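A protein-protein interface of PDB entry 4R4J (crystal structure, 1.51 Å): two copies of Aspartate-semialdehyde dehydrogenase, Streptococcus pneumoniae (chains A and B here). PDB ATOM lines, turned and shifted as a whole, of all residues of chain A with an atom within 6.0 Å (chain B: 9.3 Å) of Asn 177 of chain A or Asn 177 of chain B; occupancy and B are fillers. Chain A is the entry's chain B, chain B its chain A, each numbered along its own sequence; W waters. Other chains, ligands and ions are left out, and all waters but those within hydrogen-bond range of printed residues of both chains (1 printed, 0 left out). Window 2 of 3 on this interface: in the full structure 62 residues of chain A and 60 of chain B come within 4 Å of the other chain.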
ATOM      1  N   LEU A 172     -16.359  24.808  22.317  1.00  0.00           N
ATOM      2  CA  LEU A 172     -15.276  25.672  21.846  1.00  0.00           C
ATOM      3  C   LEU A 172     -15.793  27.034  21.383  1.00  0.00           C
ATOM      4  O   LEU A 172     -15.184  28.071  21.682  1.00  0.00           O
ATOM      5  CB  LEU A 172     -14.473  24.999  20.731  1.00  0.00           C
ATOM      6  CG  LEU A 172     -13.629  23.804  21.184  1.00  0.00           C
ATOM      7  CD1 LEU A 172     -13.256  22.910  20.003  1.00  0.00           C
ATOM      8  CD2 LEU A 172     -12.392  24.297  21.919  1.00  0.00           C
ATOM      9  N   ARG A 173     -16.915  27.032  20.661  1.00  0.00           N
ATOM     10  CA  ARG A 173     -17.514  28.289  20.222  1.00  0.00           C
ATOM     11  C   ARG A 173     -17.982  29.140  21.396  1.00  0.00           C
ATOM     12  O   ARG A 173     -17.844  30.351  21.355  1.00  0.00           O
ATOM     13  CB  ARG A 173     -18.650  28.043  19.226  1.00  0.00           C
ATOM     14  CG  ARG A 173     -18.167  27.550  17.866  1.00  0.00           C
ATOM     15  CD  ARG A 173     -19.349  27.285  16.934  1.00  0.00           C
ATOM     16  NE  ARG A 173     -18.932  26.787  15.618  1.00  0.00           N
ATOM     17  CZ  ARG A 173     -19.320  25.639  15.054  1.00  0.00           C
ATOM     18  NH1 ARG A 173     -20.183  24.815  15.652  1.00  0.00           N
ATOM     19  NH2 ARG A 173     -18.854  25.322  13.852  1.00  0.00           N
ATOM     20  N   GLU A 174     -18.537  28.525  22.437  1.00  0.00           N
ATOM     21  CA  GLU A 174     -18.939  29.289  23.626  1.00  0.00           C
ATOM     22  C   GLU A 174     -17.744  30.000  24.257  1.00  0.00           C
ATOM     23  O   GLU A 174     -17.841  31.165  24.655  1.00  0.00           O
ATOM     24  CB  GLU A 174     -19.576  28.389  24.681  1.00  0.00           C
ATOM     25  CG  GLU A 174     -20.998  27.949  24.389  1.00  0.00           C
ATOM     26  CD  GLU A 174     -21.716  27.512  25.646  1.00  0.00           C
ATOM     27  OE1 GLU A 174     -22.240  28.380  26.379  1.00  0.00           O
ATOM     28  OE2 GLU A 174     -21.734  26.303  25.912  1.00  0.00           O
ATOM     29  N   VAL A 175     -16.615  29.302  24.343  1.00  0.00           N
ATOM     30  CA  VAL A 175     -15.407  29.882  24.938  1.00  0.00           C
ATOM     31  C   VAL A 175     -14.872  30.999  24.048  1.00  0.00           C
ATOM     32  O   VAL A 175     -14.689  32.143  24.498  1.00  0.00           O
ATOM     33  CB  VAL A 175     -14.308  28.808  25.159  1.00  0.00           C
ATOM     34  CG1 VAL A 175     -13.007  29.441  25.642  1.00  0.00           C
ATOM     35  CG2 VAL A 175     -14.782  27.759  26.147  1.00  0.00           C
ATOM     36  N   LEU A 176     -14.647  30.673  22.779  1.00  0.00           N
ATOM     37  CA  LEU A 176     -14.014  31.605  21.842  1.00  0.00           C
ATOM     38  C   LEU A 176     -14.916  32.775  21.419  1.00  0.00           C
ATOM     39  O   LEU A 176     -14.429  33.889  21.249  1.00  0.00           O
ATOM     40  CB  LEU A 176     -13.510  30.862  20.599  1.00  0.00           C
ATOM     41  CG  LEU A 176     -12.310  29.933  20.819  1.00  0.00           C
ATOM     42  CD1 LEU A 176     -12.240  28.882  19.719  1.00  0.00           C
ATOM     43  CD2 LEU A 176     -11.002  30.712  20.900  1.00  0.00           C
ATOM     44  N   ASN A 177     -16.211  32.523  21.249  1.00  0.00           N
ATOM     45  CA  ASN A 177     -17.147  33.548  20.759  1.00  0.00           C
ATOM     46  C   ASN A 177     -17.905  34.293  21.850  1.00  0.00           C
ATOM     47  O   ASN A 177     -18.178  35.482  21.695  1.00  0.00           O
ATOM     48  CB  ASN A 177     -18.147  32.940  19.773  1.00  0.00           C
ATOM     49  CG  ASN A 177     -17.473  32.337  18.555  1.00  0.00           C
ATOM     50  OD1 ASN A 177     -16.346  32.698  18.207  1.00  0.00           O
ATOM     51  ND2 ASN A 177     -18.158  31.410  17.903  1.00  0.00           N
ATOM     52  N   ASP A 178     -18.250  33.599  22.935  1.00  0.00           N
ATOM     53  CA  ASP A 178     -19.016  34.196  24.037  1.00  0.00           C
ATOM     54  C   ASP A 178     -18.185  34.475  25.295  1.00  0.00           C
ATOM     55  O   ASP A 178     -18.711  35.012  26.262  1.00  0.00           O
ATOM     56  CB  ASP A 178     -20.202  33.294  24.407  1.00  0.00           C
ATOM     57  CG  ASP A 178     -21.054  32.913  23.204  1.00  0.00           C
ATOM     58  OD1 ASP A 178     -21.079  33.674  22.211  1.00  0.00           O
ATOM     59  OD2 ASP A 178     -21.709  31.846  23.257  1.00  0.00           O
ATOM     60  N   GLY A 179     -16.909  34.095  25.297  1.00  0.00           N
ATOM     61  CA  GLY A 179     -16.022  34.367  26.440  1.00  0.00           C
ATOM     62  C   GLY A 179     -16.317  33.559  27.693  1.00  0.00           C
ATOM     63  O   GLY A 179     -15.922  33.951  28.791  1.00  0.00           O
ATOM     64  N   GLN B 169      -5.910  30.710  19.330  1.00  0.00           N
ATOM     65  CA  GLN B 169      -7.276  31.242  19.301  1.00  0.00           C
ATOM     66  C   GLN B 169      -7.711  31.607  17.881  1.00  0.00           C
ATOM     67  O   GLN B 169      -8.840  31.339  17.478  1.00  0.00           O
ATOM     68  CB  GLN B 169      -7.384  32.455  20.222  1.00  0.00           C
ATOM     69  CG  GLN B 169      -7.163  32.151  21.699  1.00  0.00           C
ATOM     70  CD  GLN B 169      -7.146  33.414  22.543  1.00  0.00           C
ATOM     71  OE1 GLN B 169      -6.388  34.344  22.265  1.00  0.00           O
ATOM     72  NE2 GLN B 169      -7.974  33.454  23.577  1.00  0.00           N
ATOM     73  N   ARG B 170      -6.791  32.202  17.129  1.00  0.00           N
ATOM     74  CA  ARG B 170      -7.033  32.581  15.745  1.00  0.00           C
ATOM     75  C   ARG B 170      -7.334  31.349  14.901  1.00  0.00           C
ATOM     76  O   ARG B 170      -8.319  31.333  14.157  1.00  0.00           O
ATOM     77  CB  ARG B 170      -5.813  33.332  15.201  1.00  0.00           C
ATOM     78  CG  ARG B 170      -6.063  34.115  13.923  1.00  0.00           C
ATOM     79  CD  ARG B 170      -5.388  33.495  12.737  1.00  0.00           C
ATOM     80  NE  ARG B 170      -3.975  33.159  12.934  1.00  0.00           N
ATOM     81  CZ  ARG B 170      -3.363  32.171  12.281  1.00  0.00           C
ATOM     82  NH1 ARG B 170      -4.040  31.426  11.405  1.00  0.00           N
ATOM     83  NH2 ARG B 170      -2.081  31.913  12.500  1.00  0.00           N
ATOM     84  N   GLU B 171      -6.496  30.316  15.037  1.00  0.00           N
ATOM     85  CA  GLU B 171      -6.670  29.074  14.281  1.00  0.00           C
ATOM     86  C   GLU B 171      -8.005  28.419  14.596  1.00  0.00           C
ATOM     87  O   GLU B 171      -8.743  28.050  13.687  1.00  0.00           O
ATOM     88  CB  GLU B 171      -5.530  28.086  14.544  1.00  0.00           C
ATOM     89  CG  GLU B 171      -4.220  28.479  13.881  1.00  0.00           C
ATOM     90  CD  GLU B 171      -3.064  27.574  14.228  1.00  0.00           C
ATOM     91  OE1 GLU B 171      -3.321  26.486  14.781  1.00  0.00           O
ATOM     92  OE2 GLU B 171      -1.893  27.959  13.956  1.00  0.00           O
ATOM     93  N   LEU B 172      -8.309  28.274  15.883  1.00  0.00           N
ATOM     94  CA  LEU B 172      -9.583  27.684  16.282  1.00  0.00           C
ATOM     95  C   LEU B 172     -10.797  28.455  15.739  1.00  0.00           C
ATOM     96  O   LEU B 172     -11.766  27.844  15.286  1.00  0.00           O
ATOM     97  CB  LEU B 172      -9.672  27.543  17.798  1.00  0.00           C
ATOM     98  CG  LEU B 172      -8.734  26.479  18.387  1.00  0.00           C
ATOM     99  CD1 LEU B 172      -8.535  26.695  19.876  1.00  0.00           C
ATOM    100  CD2 LEU B 172      -9.269  25.090  18.098  1.00  0.00           C
ATOM    101  N   ARG B 173     -10.740  29.785  15.779  1.00  0.00           N
ATOM    102  CA  ARG B 173     -11.833  30.605  15.249  1.00  0.00           C
ATOM    103  C   ARG B 173     -11.994  30.412  13.737  1.00  0.00           C
ATOM    104  O   ARG B 173     -13.112  30.326  13.236  1.00  0.00           O
ATOM    105  CB  ARG B 173     -11.629  32.082  15.595  1.00  0.00           C
ATOM    106  CG  ARG B 173     -11.946  32.419  17.040  1.00  0.00           C
ATOM    107  CD  ARG B 173     -11.680  33.879  17.366  1.00  0.00           C
ATOM    108  NE  ARG B 173     -12.065  34.173  18.750  1.00  0.00           N
ATOM    109  CZ  ARG B 173     -11.265  34.661  19.703  1.00  0.00           C
ATOM    110  NH1 ARG B 173      -9.995  34.962  19.464  1.00  0.00           N
ATOM    111  NH2 ARG B 173     -11.758  34.876  20.917  1.00  0.00           N
ATOM    112  N   GLU B 174     -10.880  30.321  13.015  1.00  0.00           N
ATOM    113  CA  GLU B 174     -10.938  30.107  11.561  1.00  0.00           C
ATOM    114  C   GLU B 174     -11.622  28.774  11.245  1.00  0.00           C
ATOM    115  O   GLU B 174     -12.441  28.690  10.355  1.00  0.00           O
ATOM    116  CB  GLU B 174      -9.535  30.151  10.947  1.00  0.00           C
ATOM    117  CG  GLU B 174      -8.940  31.553  10.921  1.00  0.00           C
ATOM    118  CD  GLU B 174      -7.548  31.624  10.314  1.00  0.00           C
ATOM    119  OE1 GLU B 174      -6.924  32.694  10.407  1.00  0.00           O
ATOM    120  OE2 GLU B 174      -7.074  30.633   9.738  1.00  0.00           O
ATOM    121  N   VAL B 175     -11.302  27.738  12.003  1.00  0.00           N
ATOM    122  CA  VAL B 175     -11.927  26.441  11.793  1.00  0.00           C
ATOM    123  C   VAL B 175     -13.405  26.474  12.186  1.00  0.00           C
ATOM    124  O   VAL B 175     -14.277  26.121  11.391  1.00  0.00           O
ATOM    125  CB  VAL B 175     -11.204  25.338  12.591  1.00  0.00           C
ATOM    126  CG1 VAL B 175     -11.953  24.012  12.471  1.00  0.00           C
ATOM    127  CG2 VAL B 175      -9.764  25.191  12.110  1.00  0.00           C
ATOM    128  N   LEU B 176     -13.680  26.941  13.398  1.00  0.00           N
ATOM    129  CA  LEU B 176     -15.013  26.823  13.992  1.00  0.00           C
ATOM    130  C   LEU B 176     -16.025  27.802  13.423  1.00  0.00           C
ATOM    131  O   LEU B 176     -17.212  27.485  13.338  1.00  0.00           O
ATOM    132  CB  LEU B 176     -14.921  27.009  15.501  1.00  0.00           C
ATOM    133  CG  LEU B 176     -14.252  25.829  16.203  1.00  0.00           C
ATOM    134  CD1 LEU B 176     -13.707  26.265  17.548  1.00  0.00           C
ATOM    135  CD2 LEU B 176     -15.208  24.660  16.363  1.00  0.00           C
ATOM    136  N   ASN B 177     -15.555  28.993  13.059  1.00  0.00           N
ATOM    137  CA  ASN B 177     -16.432  30.051  12.580  1.00  0.00           C
ATOM    138  C   ASN B 177     -16.394  30.243  11.074  1.00  0.00           C
ATOM    139  O   ASN B 177     -17.405  30.626  10.485  1.00  0.00           O
ATOM    140  CB  ASN B 177     -16.086  31.365  13.275  1.00  0.00           C
ATOM    141  CG  ASN B 177     -16.260  31.283  14.774  1.00  0.00           C
ATOM    142  OD1 ASN B 177     -17.060  30.488  15.272  1.00  0.00           O
ATOM    143  ND2 ASN B 177     -15.532  32.122  15.505  1.00  0.00           N
ATOM    144  N   ASP B 178     -15.235  30.014  10.456  1.00  0.00           N
ATOM    145  CA  ASP B 178     -15.091  30.223   9.007  1.00  0.00           C
ATOM    146  C   ASP B 178     -15.049  28.928   8.174  1.00  0.00           C
ATOM    147  O   ASP B 178     -15.055  28.986   6.943  1.00  0.00           O
ATOM    148  CB  ASP B 178     -13.838  31.049   8.719  1.00  0.00           C
ATOM    149  CG  ASP B 178     -13.832  32.388   9.446  1.00  0.00           C
ATOM    150  OD1 ASP B 178     -14.922  32.922   9.749  1.00  0.00           O
ATOM    151  OD2 ASP B 178     -12.725  32.906   9.715  1.00  0.00           O
ATOM    152  N   GLY B 179     -14.990  27.772   8.833  1.00  0.00           N
ATOM    153  CA  GLY B 179     -15.005  26.481   8.143  1.00  0.00           C
ATOM    154  C   GLY B 179     -13.691  26.076   7.491  1.00  0.00           C
ATOM    155  O   GLY B 179     -13.670  25.205   6.626  1.00  0.00           O
ATOM    156  N   VAL B 180     -12.587  26.677   7.922  1.00  0.00           N
ATOM    157  CA  VAL B 180     -11.267  26.332   7.394  1.00  0.00           C
ATOM    158  C   VAL B 180     -10.895  24.924   7.871  1.00  0.00           C
ATOM    159  O   VAL B 180     -11.163  24.567   9.015  1.00  0.00           O
ATOM    160  CB  VAL B 180     -10.202  27.358   7.855  1.00  0.00           C
ATOM    161  CG1 VAL B 180      -8.808  26.976   7.365  1.00  0.00           C
ATOM    162  CG2 VAL B 180     -10.563  28.754   7.361  1.00  0.00           C
ATOM    163  N   PHE B 203      -6.956  21.506  16.751  1.00  0.00           N
ATOM    164  CA  PHE B 203      -7.362  20.107  16.553  1.00  0.00           C
ATOM    165  C   PHE B 203      -6.188  19.171  16.227  1.00  0.00           C
ATOM    166  O   PHE B 203      -6.353  18.158  15.520  1.00  0.00           O
ATOM    167  CB  PHE B 203      -8.481  20.021  15.509  1.00  0.00           C
ATOM    168  CG  PHE B 203      -9.672  20.863  15.856  1.00  0.00           C
ATOM    169  CD1 PHE B 203     -10.555  20.451  16.834  1.00  0.00           C
ATOM    170  CD2 PHE B 203      -9.883  22.099  15.244  1.00  0.00           C
ATOM    171  CE1 PHE B 203     -11.649  21.227  17.179  1.00  0.00           C
ATOM    172  CE2 PHE B 203     -10.975  22.880  15.588  1.00  0.00           C
ATOM    173  CZ  PHE B 203     -11.861  22.439  16.556  1.00  0.00           C
HETATM  174  O   HOH W   1     -14.835  34.999  18.325  1.00  0.00           O
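The side-chain amide nitrogen (ND2) of Asn 177 of chain B sits at hydrogen-bond distance from the side-chain amide oxygen (OD1) of Asn 177 of chain A. The backbone carbonyl oxygen (O) of Leu 176 of chain B lies within hydrogen-bond range of the guanidinium group (NH2) of Arg 173 of chain A (2.8 Å). O of Leu 176 of chain A is in hydrogen-bond range of NH2 of Arg 173 of chain B (2.9 Å).
CD1 of Leu 176 of chain B touches CB of Leu 172 of chain A (3.5 Å). Leu 172 of chain A touches Phe 203 of chain B (CD1 to CE1, 3.7 Å). Leu 172 of chain B touches Leu 176 of chain A (CB to CD1, 3.5 Å). Leu 176 of chain B touches Leu 176 of chain A.
Printed residues of chain B within 4 Å of Leu 172 of chain A: Leu 176 and Phe 203. Printed residues of chain B within 4 Å of Leu 176 of chain A: Leu 172, Arg 173 and Leu 176. Of chain B, only Asn 177 (2.9 Å) comes within 4 Å of Asn 177 of chain A. Gln 169 of chain B touches none of the printed residues of chain A. Of the printed residues of chain A, Leu 172 of chain B touches Leu 176 (3.5 Å). Printed residues of chain A within 4 Å of Arg 173 of chain B: Leu 176 (2.9 Å). Printed residues of chain A within 4 Å of Leu 176 of chain B: Leu 172 (3.5 Å), Arg 173 (2.8 Å) and Leu 176 (3.7 Å). The nearest residue of chain B that does not touch Asn 177 of chain A is Arg 173 of chain B (4.6 Å). The nearest residue of chain A that does not touch Asn 177 of chain B is Arg 173 of chain A (4.1 Å).
Of the 13 printed residues of chain B, 5 touch a printed residue of chain A. Hydrophobic or aromatic side chains of chain B that line the printed part of chain A: Leu 172, Leu 176 and Phe 203. Of the 8 printed residues of chain A, 4 touch a printed residue of chain B. Among the printed residues, 7 pairs touch across the chains. Among the printed residues, no Asp or Glu carboxylate lies within 4 Å of a Lys or Arg side-chain nitrogen of the other chain.
Leu 172 of chain A touches Leu 176 of chain B, and with the chains exchanged Leu 176 of chain A touches Leu 172 of chain B. Arg 173 of chain A touches Leu 176 of chain B, and with the chains exchanged Leu 176 of chain A touches Arg 173 of chain B. Leu 176 of chain A touches its own counterpart, Leu 176 of chain B. Asn 177 of chain B touches its own counterpart, Asn 177 of chain A. Positions printed for both chains: 172, 173, 174, 175, 176, 177, 178 and 179.
Water W1 lies within hydrogen-bond range of the side-chain amide oxygen (OD1) of Asn 177 of chain A (2.8 Å), the guanidinium group (NE) of Arg 173 of chain B (2.9 Å) and the backbone carbonyl oxygen (O) of Leu 176 of chain A (3.2 Å).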
